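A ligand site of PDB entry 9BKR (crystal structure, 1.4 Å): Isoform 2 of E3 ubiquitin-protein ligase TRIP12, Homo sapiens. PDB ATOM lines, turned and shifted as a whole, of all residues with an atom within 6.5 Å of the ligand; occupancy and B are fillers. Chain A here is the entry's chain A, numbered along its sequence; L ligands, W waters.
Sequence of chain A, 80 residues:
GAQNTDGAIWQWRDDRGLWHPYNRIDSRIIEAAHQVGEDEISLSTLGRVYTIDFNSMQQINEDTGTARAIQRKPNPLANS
NH2 of Arg 48 is in salt-bridge range of O3 of the ligand (2.5 Å).
The side-chain hydroxyl (OG1) of Thr 66 lies within hydrogen-bond range of an oxygen (O5) of the ligand (2.6 Å).
OH of Tyr 50 is in hydrogen-bond range of O8 of the ligand.
O7 of the ligand is in salt-bridge range of NE of Arg 68 (2.7 Å).
O5 of the ligand lies within hydrogen-bond range of OG1 of Thr 64, at 2.7 Å.
ND2 of Asn 61 lies within hydrogen-bond range of O8 of the ligand, 2.8 Å away.
The side-chain amide oxygen of Gln 59 lies within hydrogen-bond range of a nitrogen (N3) of the ligand (2.9 Å).
The side-chain hydroxyl of Thr 64 sits at hydrogen-bond distance from the backbone NH of Thr 66, at 3.2 Å.
The backbone carbonyl oxygen (O) of Thr 66 lies within hydrogen-bond range of the backbone NH (N) of Asn 61 (2.9 Å).
N of Leu 43 sits at hydrogen-bond distance from O of Tyr 50 (2.8 Å).
The backbone NH (N) of Gln 59 sits at hydrogen-bond distance from the backbone carbonyl oxygen (O) of Arg 68 (2.8 Å).
The guanidinium group of Arg 68 lies within salt-bridge range of the side-chain carboxylate of Asp 15 (2.6 Å).
The backbone carbonyl oxygen (O) of Arg 13 is in hydrogen-bond range of the guanidinium group (NH1) of Arg 68 (3.2 Å).
The side-chain hydroxyl of Tyr 22 lies within hydrogen-bond range of the side-chain amide oxygen of Gln 59.
O of Trp 12 is in hydrogen-bond range of N of His 20 (2.9 Å).
Water W4 lies within hydrogen-bond range of an oxygen (O13) of the ligand (2.5 Å) and the backbone NH of Asp 15 (2.8 Å).
Water W3 lies within hydrogen-bond range of O7 of the ligand (2.7 Å), NE2 of Gln 59 (3.0 Å) and O of Thr 66 (3.1 Å).
NE1 of Trp 12 lies close to N3 of the ligand (3.5 Å).
Tyr 22 touches the ligand (CE1 to N3, 3.5 Å).
Leu 46 touches the ligand.
Hydrophobic or aromatic side chains within 4 Å of the ligand: Trp 12, Tyr 22, Leu 46 and Tyr 50.
The nearest printed residue that does not touch the ligand is Asp 14 (4.1 Å).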
ATOM      1  N   TRP A  12      14.326 -17.793 -24.185  1.00  0.00           N
ATOM      2  CA  TRP A  12      15.462 -17.285 -23.434  1.00  0.00           C
ATOM      3  C   TRP A  12      15.758 -18.202 -22.231  1.00  0.00           C
ATOM      4  O   TRP A  12      14.874 -18.890 -21.735  1.00  0.00           O
ATOM      5  CB  TRP A  12      15.209 -15.842 -22.980  1.00  0.00           C
ATOM      6  CG  TRP A  12      13.965 -15.677 -22.141  1.00  0.00           C
ATOM      7  CD1 TRP A  12      12.701 -15.435 -22.574  1.00  0.00           C
ATOM      8  CD2 TRP A  12      13.897 -15.726 -20.704  1.00  0.00           C
ATOM      9  NE1 TRP A  12      11.839 -15.333 -21.505  1.00  0.00           N
ATOM     10  CE2 TRP A  12      12.554 -15.521 -20.356  1.00  0.00           C
ATOM     11  CE3 TRP A  12      14.841 -15.932 -19.700  1.00  0.00           C
ATOM     12  CZ2 TRP A  12      12.114 -15.510 -19.043  1.00  0.00           C
ATOM     13  CZ3 TRP A  12      14.420 -15.915 -18.386  1.00  0.00           C
ATOM     14  CH2 TRP A  12      13.072 -15.719 -18.068  1.00  0.00           C
ATOM     15  N   ARG A  13      17.027 -18.209 -21.806  1.00  0.00           N
ATOM     16  CA  ARG A  13      17.480 -19.137 -20.772  1.00  0.00           C
ATOM     17  C   ARG A  13      17.595 -18.438 -19.399  1.00  0.00           C
ATOM     18  O   ARG A  13      18.265 -17.416 -19.276  1.00  0.00           O
ATOM     19  CB  ARG A  13      18.793 -19.778 -21.210  1.00  0.00           C
ATOM     20  CG  ARG A  13      19.089 -21.090 -20.515  1.00  0.00           C
ATOM     21  CD  ARG A  13      20.427 -21.650 -20.914  1.00  0.00           C
ATOM     22  NE  ARG A  13      20.442 -23.081 -20.602  1.00  0.00           N
ATOM     23  CZ  ARG A  13      21.445 -23.881 -20.830  1.00  0.00           C
ATOM     24  NH1 ARG A  13      21.358 -25.143 -20.415  1.00  0.00           N
ATOM     25  NH2 ARG A  13      22.512 -23.438 -21.483  1.00  0.00           N
ATOM     26  N   ASP A  14      16.934 -19.031 -18.380  1.00  0.00           N
ATOM     27  CA  ASP A  14      16.965 -18.460 -17.046  1.00  0.00           C
ATOM     28  C   ASP A  14      18.251 -18.871 -16.336  1.00  0.00           C
ATOM     29  O   ASP A  14      19.061 -19.626 -16.853  1.00  0.00           O
ATOM     30  CB  ASP A  14      15.677 -18.789 -16.297  1.00  0.00           C
ATOM     31  CG  ASP A  14      15.502 -20.227 -15.849  1.00  0.00           C
ATOM     32  OD1 ASP A  14      16.522 -20.957 -15.820  1.00  0.00           O
ATOM     33  OD2 ASP A  14      14.349 -20.605 -15.565  1.00  0.00           O
ATOM     34  N   ASP A  15      18.403 -18.389 -15.098  1.00  0.00           N
ATOM     35  CA  ASP A  15      19.655 -18.550 -14.374  1.00  0.00           C
ATOM     36  C   ASP A  15      19.871 -20.023 -14.062  1.00  0.00           C
ATOM     37  O   ASP A  15      21.019 -20.482 -14.027  1.00  0.00           O
ATOM     38  CB  ASP A  15      19.641 -17.738 -13.088  1.00  0.00           C
ATOM     39  CG  ASP A  15      19.634 -16.231 -13.280  1.00  0.00           C
ATOM     40  OD1 ASP A  15      20.102 -15.787 -14.341  1.00  0.00           O
ATOM     41  OD2 ASP A  15      19.232 -15.481 -12.333  1.00  0.00           O
ATOM     42  N   HIS A  20      12.516 -20.491 -21.495  1.00  0.00           N
ATOM     43  CA  HIS A  20      11.205 -19.883 -21.401  1.00  0.00           C
ATOM     44  C   HIS A  20      10.809 -19.286 -22.750  1.00  0.00           C
ATOM     45  O   HIS A  20      11.592 -18.543 -23.346  1.00  0.00           O
ATOM     46  CB  HIS A  20      11.258 -18.740 -20.401  1.00  0.00           C
ATOM     47  CG  HIS A  20      11.568 -19.161 -19.021  1.00  0.00           C
ATOM     48  ND1 HIS A  20      10.559 -19.448 -18.153  1.00  0.00           N
ATOM     49  CD2 HIS A  20      12.691 -19.448 -18.405  1.00  0.00           C
ATOM     50  CE1 HIS A  20      11.100 -19.796 -16.988  1.00  0.00           C
ATOM     51  NE2 HIS A  20      12.406 -19.808 -17.124  1.00  0.00           N
ATOM     52  N   TYR A  22       9.456 -16.575 -25.172  1.00  0.00           N
ATOM     53  CA  TYR A  22       8.968 -15.209 -25.278  1.00  0.00           C
ATOM     54  C   TYR A  22       7.467 -15.241 -25.568  1.00  0.00           C
ATOM     55  O   TYR A  22       6.964 -16.245 -26.051  1.00  0.00           O
ATOM     56  CB  TYR A  22       9.744 -14.479 -26.381  1.00  0.00           C
ATOM     57  CG  TYR A  22      11.174 -14.082 -26.044  1.00  0.00           C
ATOM     58  CD1 TYR A  22      11.453 -12.943 -25.296  1.00  0.00           C
ATOM     59  CD2 TYR A  22      12.255 -14.860 -26.481  1.00  0.00           C
ATOM     60  CE1 TYR A  22      12.752 -12.569 -25.038  1.00  0.00           C
ATOM     61  CE2 TYR A  22      13.558 -14.503 -26.209  1.00  0.00           C
ATOM     62  CZ  TYR A  22      13.815 -13.360 -25.464  1.00  0.00           C
ATOM     63  OH  TYR A  22      15.110 -13.043 -25.216  1.00  0.00           O
ATOM     64  N   ASP A  26       6.618 -10.731 -28.709  1.00  0.00           N
ATOM     65  CA  ASP A  26       8.066 -10.593 -28.615  1.00  0.00           C
ATOM     66  C   ASP A  26       8.748 -11.586 -29.559  1.00  0.00           C
ATOM     67  O   ASP A  26       9.750 -11.251 -30.189  1.00  0.00           O
ATOM     68  CB  ASP A  26       8.529 -10.634 -27.166  1.00  0.00           C
ATOM     69  CG  ASP A  26       8.230  -9.370 -26.361  1.00  0.00           C
ATOM     70  OD1 ASP A  26       7.949  -8.313 -26.980  1.00  0.00           O
ATOM     71  OD2 ASP A  26       8.312  -9.437 -25.113  1.00  0.00           O
ATOM     72  N   LEU A  43      14.247  -4.611 -27.255  1.00  0.00           N
ATOM     73  CA  LEU A  43      12.978  -5.171 -26.848  1.00  0.00           C
ATOM     74  C   LEU A  43      12.689  -4.638 -25.445  1.00  0.00           C
ATOM     75  O   LEU A  43      13.589  -4.641 -24.604  1.00  0.00           O
ATOM     76  CB  LEU A  43      13.240  -6.685 -26.872  1.00  0.00           C
ATOM     77  CG  LEU A  43      12.038  -7.617 -26.873  1.00  0.00           C
ATOM     78  CD1 LEU A  43      11.295  -7.496 -28.168  1.00  0.00           C
ATOM     79  CD2 LEU A  43      12.422  -9.065 -26.642  1.00  0.00           C
ATOM     80  N   THR A  45      10.328  -5.361 -22.161  1.00  0.00           N
ATOM     81  CA  THR A  45       9.316  -6.115 -21.444  1.00  0.00           C
ATOM     82  C   THR A  45       9.546  -5.919 -19.947  1.00  0.00           C
ATOM     83  O   THR A  45      10.684  -5.768 -19.514  1.00  0.00           O
ATOM     84  CB  THR A  45       9.385  -7.582 -21.881  1.00  0.00           C
ATOM     85  OG1 THR A  45       8.321  -8.275 -21.248  1.00  0.00           O
ATOM     86  CG2 THR A  45      10.699  -8.247 -21.528  1.00  0.00           C
ATOM     87  N   LEU A  46       8.434  -5.816 -19.198  1.00  0.00           N
ATOM     88  CA  LEU A  46       8.428  -5.726 -17.739  1.00  0.00           C
ATOM     89  C   LEU A  46       9.148  -4.462 -17.265  1.00  0.00           C
ATOM     90  O   LEU A  46       9.587  -4.393 -16.111  1.00  0.00           O
ATOM     91  CB  LEU A  46       9.048  -6.971 -17.129  1.00  0.00           C
ATOM     92  CG  LEU A  46       8.315  -8.288 -17.418  1.00  0.00           C
ATOM     93  CD1 LEU A  46       9.079  -9.458 -16.790  1.00  0.00           C
ATOM     94  CD2 LEU A  46       6.888  -8.245 -16.905  1.00  0.00           C
ATOM     95  N   ARG A  48      11.878  -3.393 -18.482  1.00  0.00           N
ATOM     96  CA  ARG A  48      13.283  -3.628 -18.638  1.00  0.00           C
ATOM     97  C   ARG A  48      13.589  -3.382 -20.098  1.00  0.00           C
ATOM     98  O   ARG A  48      12.670  -3.393 -20.928  1.00  0.00           O
ATOM     99  CB  ARG A  48      13.647  -5.048 -18.188  1.00  0.00           C
ATOM    100  CG  ARG A  48      13.230  -5.332 -16.759  1.00  0.00           C
ATOM    101  CD  ARG A  48      14.284  -6.125 -16.049  1.00  0.00           C
ATOM    102  NE  ARG A  48      13.897  -6.524 -14.683  1.00  0.00           N
ATOM    103  CZ  ARG A  48      14.771  -6.921 -13.775  1.00  0.00           C
ATOM    104  NH1 ARG A  48      14.373  -7.421 -12.628  1.00  0.00           N
ATOM    105  NH2 ARG A  48      16.063  -6.808 -14.033  1.00  0.00           N
ATOM    106  N   TYR A  50      16.055  -4.665 -23.121  1.00  0.00           N
ATOM    107  CA  TYR A  50      16.955  -5.709 -23.573  1.00  0.00           C
ATOM    108  C   TYR A  50      17.430  -5.416 -24.985  1.00  0.00           C
ATOM    109  O   TYR A  50      16.689  -4.891 -25.826  1.00  0.00           O
ATOM    110  CB  TYR A  50      16.238  -7.055 -23.533  1.00  0.00           C
ATOM    111  CG  TYR A  50      15.849  -7.523 -22.143  1.00  0.00           C
ATOM    112  CD1 TYR A  50      16.810  -7.930 -21.239  1.00  0.00           C
ATOM    113  CD2 TYR A  50      14.510  -7.688 -21.789  1.00  0.00           C
ATOM    114  CE1 TYR A  50      16.474  -8.334 -19.947  1.00  0.00           C
ATOM    115  CE2 TYR A  50      14.165  -8.122 -20.523  1.00  0.00           C
ATOM    116  CZ  TYR A  50      15.147  -8.493 -19.623  1.00  0.00           C
ATOM    117  OH  TYR A  50      14.812  -8.959 -18.370  1.00  0.00           O
ATOM    118  N   GLN A  59      20.342 -12.439 -25.255  1.00  0.00           N
ATOM    119  CA  GLN A  59      19.564 -11.334 -24.733  1.00  0.00           C
ATOM    120  C   GLN A  59      20.400 -10.633 -23.657  1.00  0.00           C
ATOM    121  O   GLN A  59      20.910 -11.315 -22.769  1.00  0.00           O
ATOM    122  CB  GLN A  59      18.301 -11.860 -24.074  1.00  0.00           C
ATOM    123  CG  GLN A  59      17.491 -10.762 -23.422  1.00  0.00           C
ATOM    124  CD  GLN A  59      16.440 -11.313 -22.495  1.00  0.00           C
ATOM    125  OE1 GLN A  59      15.325 -11.654 -22.906  1.00  0.00           O
ATOM    126  NE2 GLN A  59      16.778 -11.375 -21.207  1.00  0.00           N
ATOM    127  N   ILE A  60      20.606  -9.327 -23.814  1.00  0.00           N
ATOM    128  CA  ILE A  60      21.475  -8.567 -22.921  1.00  0.00           C
ATOM    129  C   ILE A  60      20.639  -7.512 -22.202  1.00  0.00           C
ATOM    130  O   ILE A  60      20.017  -6.672 -22.852  1.00  0.00           O
ATOM    131  CB  ILE A  60      22.618  -7.886 -23.684  1.00  0.00           C
ATOM    132  CG1 ILE A  60      23.407  -8.881 -24.537  1.00  0.00           C
ATOM    133  CG2 ILE A  60      23.508  -7.080 -22.714  1.00  0.00           C
ATOM    134  CD1 ILE A  60      24.243  -8.216 -25.626  1.00  0.00           C
ATOM    135  N   ASN A  61      20.683  -7.520 -20.848  1.00  0.00           N
ATOM    136  CA  ASN A  61      20.091  -6.460 -20.070  1.00  0.00           C
ATOM    137  C   ASN A  61      21.054  -5.284 -20.076  1.00  0.00           C
ATOM    138  O   ASN A  61      22.157  -5.399 -19.562  1.00  0.00           O
ATOM    139  CB  ASN A  61      19.826  -6.931 -18.659  1.00  0.00           C
ATOM    140  CG  ASN A  61      19.146  -5.884 -17.799  1.00  0.00           C
ATOM    141  OD1 ASN A  61      19.494  -4.698 -17.867  1.00  0.00           O
ATOM    142  ND2 ASN A  61      18.156  -6.307 -17.024  1.00  0.00           N
ATOM    143  N   THR A  64      22.195  -3.990 -16.395  1.00  0.00           N
ATOM    144  CA  THR A  64      22.960  -4.832 -15.484  1.00  0.00           C
ATOM    145  C   THR A  64      24.148  -5.497 -16.175  1.00  0.00           C
ATOM    146  O   THR A  64      25.060  -5.976 -15.502  1.00  0.00           O
ATOM    147  CB  THR A  64      22.091  -5.907 -14.842  1.00  0.00           C
ATOM    148  OG1 THR A  64      21.720  -6.819 -15.860  1.00  0.00           O
ATOM    149  CG2 THR A  64      20.810  -5.356 -14.245  1.00  0.00           C
ATOM    150  N   GLY A  65      24.082  -5.597 -17.510  1.00  0.00           N
ATOM    151  CA  GLY A  65      25.100  -6.288 -18.296  1.00  0.00           C
ATOM    152  C   GLY A  65      24.934  -7.810 -18.315  1.00  0.00           C
ATOM    153  O   GLY A  65      25.787  -8.521 -18.875  1.00  0.00           O
ATOM    154  N   THR A  66      23.808  -8.325 -17.801  1.00  0.00           N
ATOM    155  CA  THR A  66      23.584  -9.762 -17.806  1.00  0.00           C
ATOM    156  C   THR A  66      23.176 -10.206 -19.207  1.00  0.00           C
ATOM    157  O   THR A  66      22.202  -9.695 -19.773  1.00  0.00           O
ATOM    158  CB  THR A  66      22.546 -10.186 -16.769  1.00  0.00           C
ATOM    159  OG1 THR A  66      23.065  -9.906 -15.460  1.00  0.00           O
ATOM    160  CG2 THR A  66      22.221 -11.673 -16.863  1.00  0.00           C
ATOM    161  N   ALA A  67      23.908 -11.194 -19.720  1.00  0.00           N
ATOM    162  CA  ALA A  67      23.651 -11.834 -21.004  1.00  0.00           C
ATOM    163  C   ALA A  67      23.142 -13.263 -20.798  1.00  0.00           C
ATOM    164  O   ALA A  67      23.705 -14.020 -20.010  1.00  0.00           O
ATOM    165  CB  ALA A  67      24.919 -11.877 -21.812  1.00  0.00           C
ATOM    166  N   ARG A  68      22.040 -13.581 -21.511  1.00  0.00           N
ATOM    167  CA  ARG A  68      21.363 -14.877 -21.485  1.00  0.00           C
ATOM    168  C   ARG A  68      21.297 -15.485 -22.889  1.00  0.00           C
ATOM    169  O   ARG A  68      21.069 -14.770 -23.863  1.00  0.00           O
ATOM    170  CB  ARG A  68      19.923 -14.686 -20.963  1.00  0.00           C
ATOM    171  CG  ARG A  68      19.847 -14.254 -19.514  1.00  0.00           C
ATOM    172  CD  ARG A  68      18.436 -13.964 -19.050  1.00  0.00           C
ATOM    173  NE  ARG A  68      18.442 -13.503 -17.655  1.00  0.00           N
ATOM    174  CZ  ARG A  68      18.760 -14.262 -16.617  1.00  0.00           C
ATOM    175  NH1 ARG A  68      18.961 -15.553 -16.790  1.00  0.00           N
ATOM    176  NH2 ARG A  68      18.885 -13.712 -15.418  1.00  0.00           N
HETATM  177  P1  LIG L   1      18.711  -8.214 -11.755  1.00  0.00           P
HETATM  178  O1  LIG L   1      17.900  -8.826 -10.652  1.00  0.00           O
HETATM  179  O2  LIG L   1      20.100  -7.807 -11.251  1.00  0.00           O
HETATM  180  O3  LIG L   1      18.001  -7.093 -12.467  1.00  0.00           O
HETATM  181  P2  LIG L   1      19.774  -9.700 -14.085  1.00  0.00           P
HETATM  182  O4  LIG L   1      19.868 -11.188 -14.079  1.00  0.00           O
HETATM  183  O5  LIG L   1      21.004  -8.863 -14.194  1.00  0.00           O
HETATM  184  O6  LIG L   1      18.933  -9.355 -12.794  1.00  0.00           O
HETATM  185  P3  LIG L   1      17.798  -9.963 -16.256  1.00  0.00           P
HETATM  186  O7  LIG L   1      18.559 -10.824 -17.224  1.00  0.00           O
HETATM  187  O8  LIG L   1      16.944  -8.858 -16.750  1.00  0.00           O
HETATM  188  O9  LIG L   1      18.774  -9.225 -15.227  1.00  0.00           O
HETATM  189  O10 LIG L   1      16.896 -10.940 -15.361  1.00  0.00           O
HETATM  190  C1  LIG L   1      16.070 -10.425 -14.299  1.00  0.00           C
HETATM  191  C2  LIG L   1      14.970 -11.407 -14.015  1.00  0.00           C
HETATM  192  O11 LIG L   1      14.082 -11.448 -15.165  1.00  0.00           O
HETATM  193  C3  LIG L   1      15.386 -12.869 -13.745  1.00  0.00           C
HETATM  194  O12 LIG L   1      14.487 -13.503 -12.848  1.00  0.00           O
HETATM  195  C4  LIG L   1      15.287 -13.474 -15.145  1.00  0.00           C
HETATM  196  O13 LIG L   1      15.104 -14.876 -15.140  1.00  0.00           O
HETATM  197  C5  LIG L   1      14.078 -12.737 -15.703  1.00  0.00           C
HETATM  198  N1  LIG L   1      14.103 -12.569 -17.172  1.00  0.00           N
HETATM  199  C6  LIG L   1      15.181 -12.395 -17.974  1.00  0.00           C
HETATM  200  N2  LIG L   1      14.845 -12.242 -19.240  1.00  0.00           N
HETATM  201  C7  LIG L   1      13.467 -12.255 -19.255  1.00  0.00           C
HETATM  202  C8  LIG L   1      12.505 -12.124 -20.278  1.00  0.00           C
HETATM  203  N3  LIG L   1      12.807 -11.996 -21.569  1.00  0.00           N
HETATM  204  N4  LIG L   1      11.197 -12.217 -19.923  1.00  0.00           N
HETATM  205  C9  LIG L   1      10.896 -12.352 -18.620  1.00  0.00           C
HETATM  206  N5  LIG L   1      11.697 -12.511 -17.576  1.00  0.00           N
HETATM  207  C10 LIG L   1      12.991 -12.432 -17.972  1.00  0.00           C
HETATM  208  O   HOH W   1      12.688 -16.052 -14.129  1.00  0.00           O
HETATM  209  O   HOH W   2      18.176  -4.267 -12.316  1.00  0.00           O
HETATM  210  O   HOH W   3      19.306 -10.652 -19.828  1.00  0.00           O
HETATM  211  O   HOH W   4      16.772 -16.380 -13.974  1.00  0.00           O
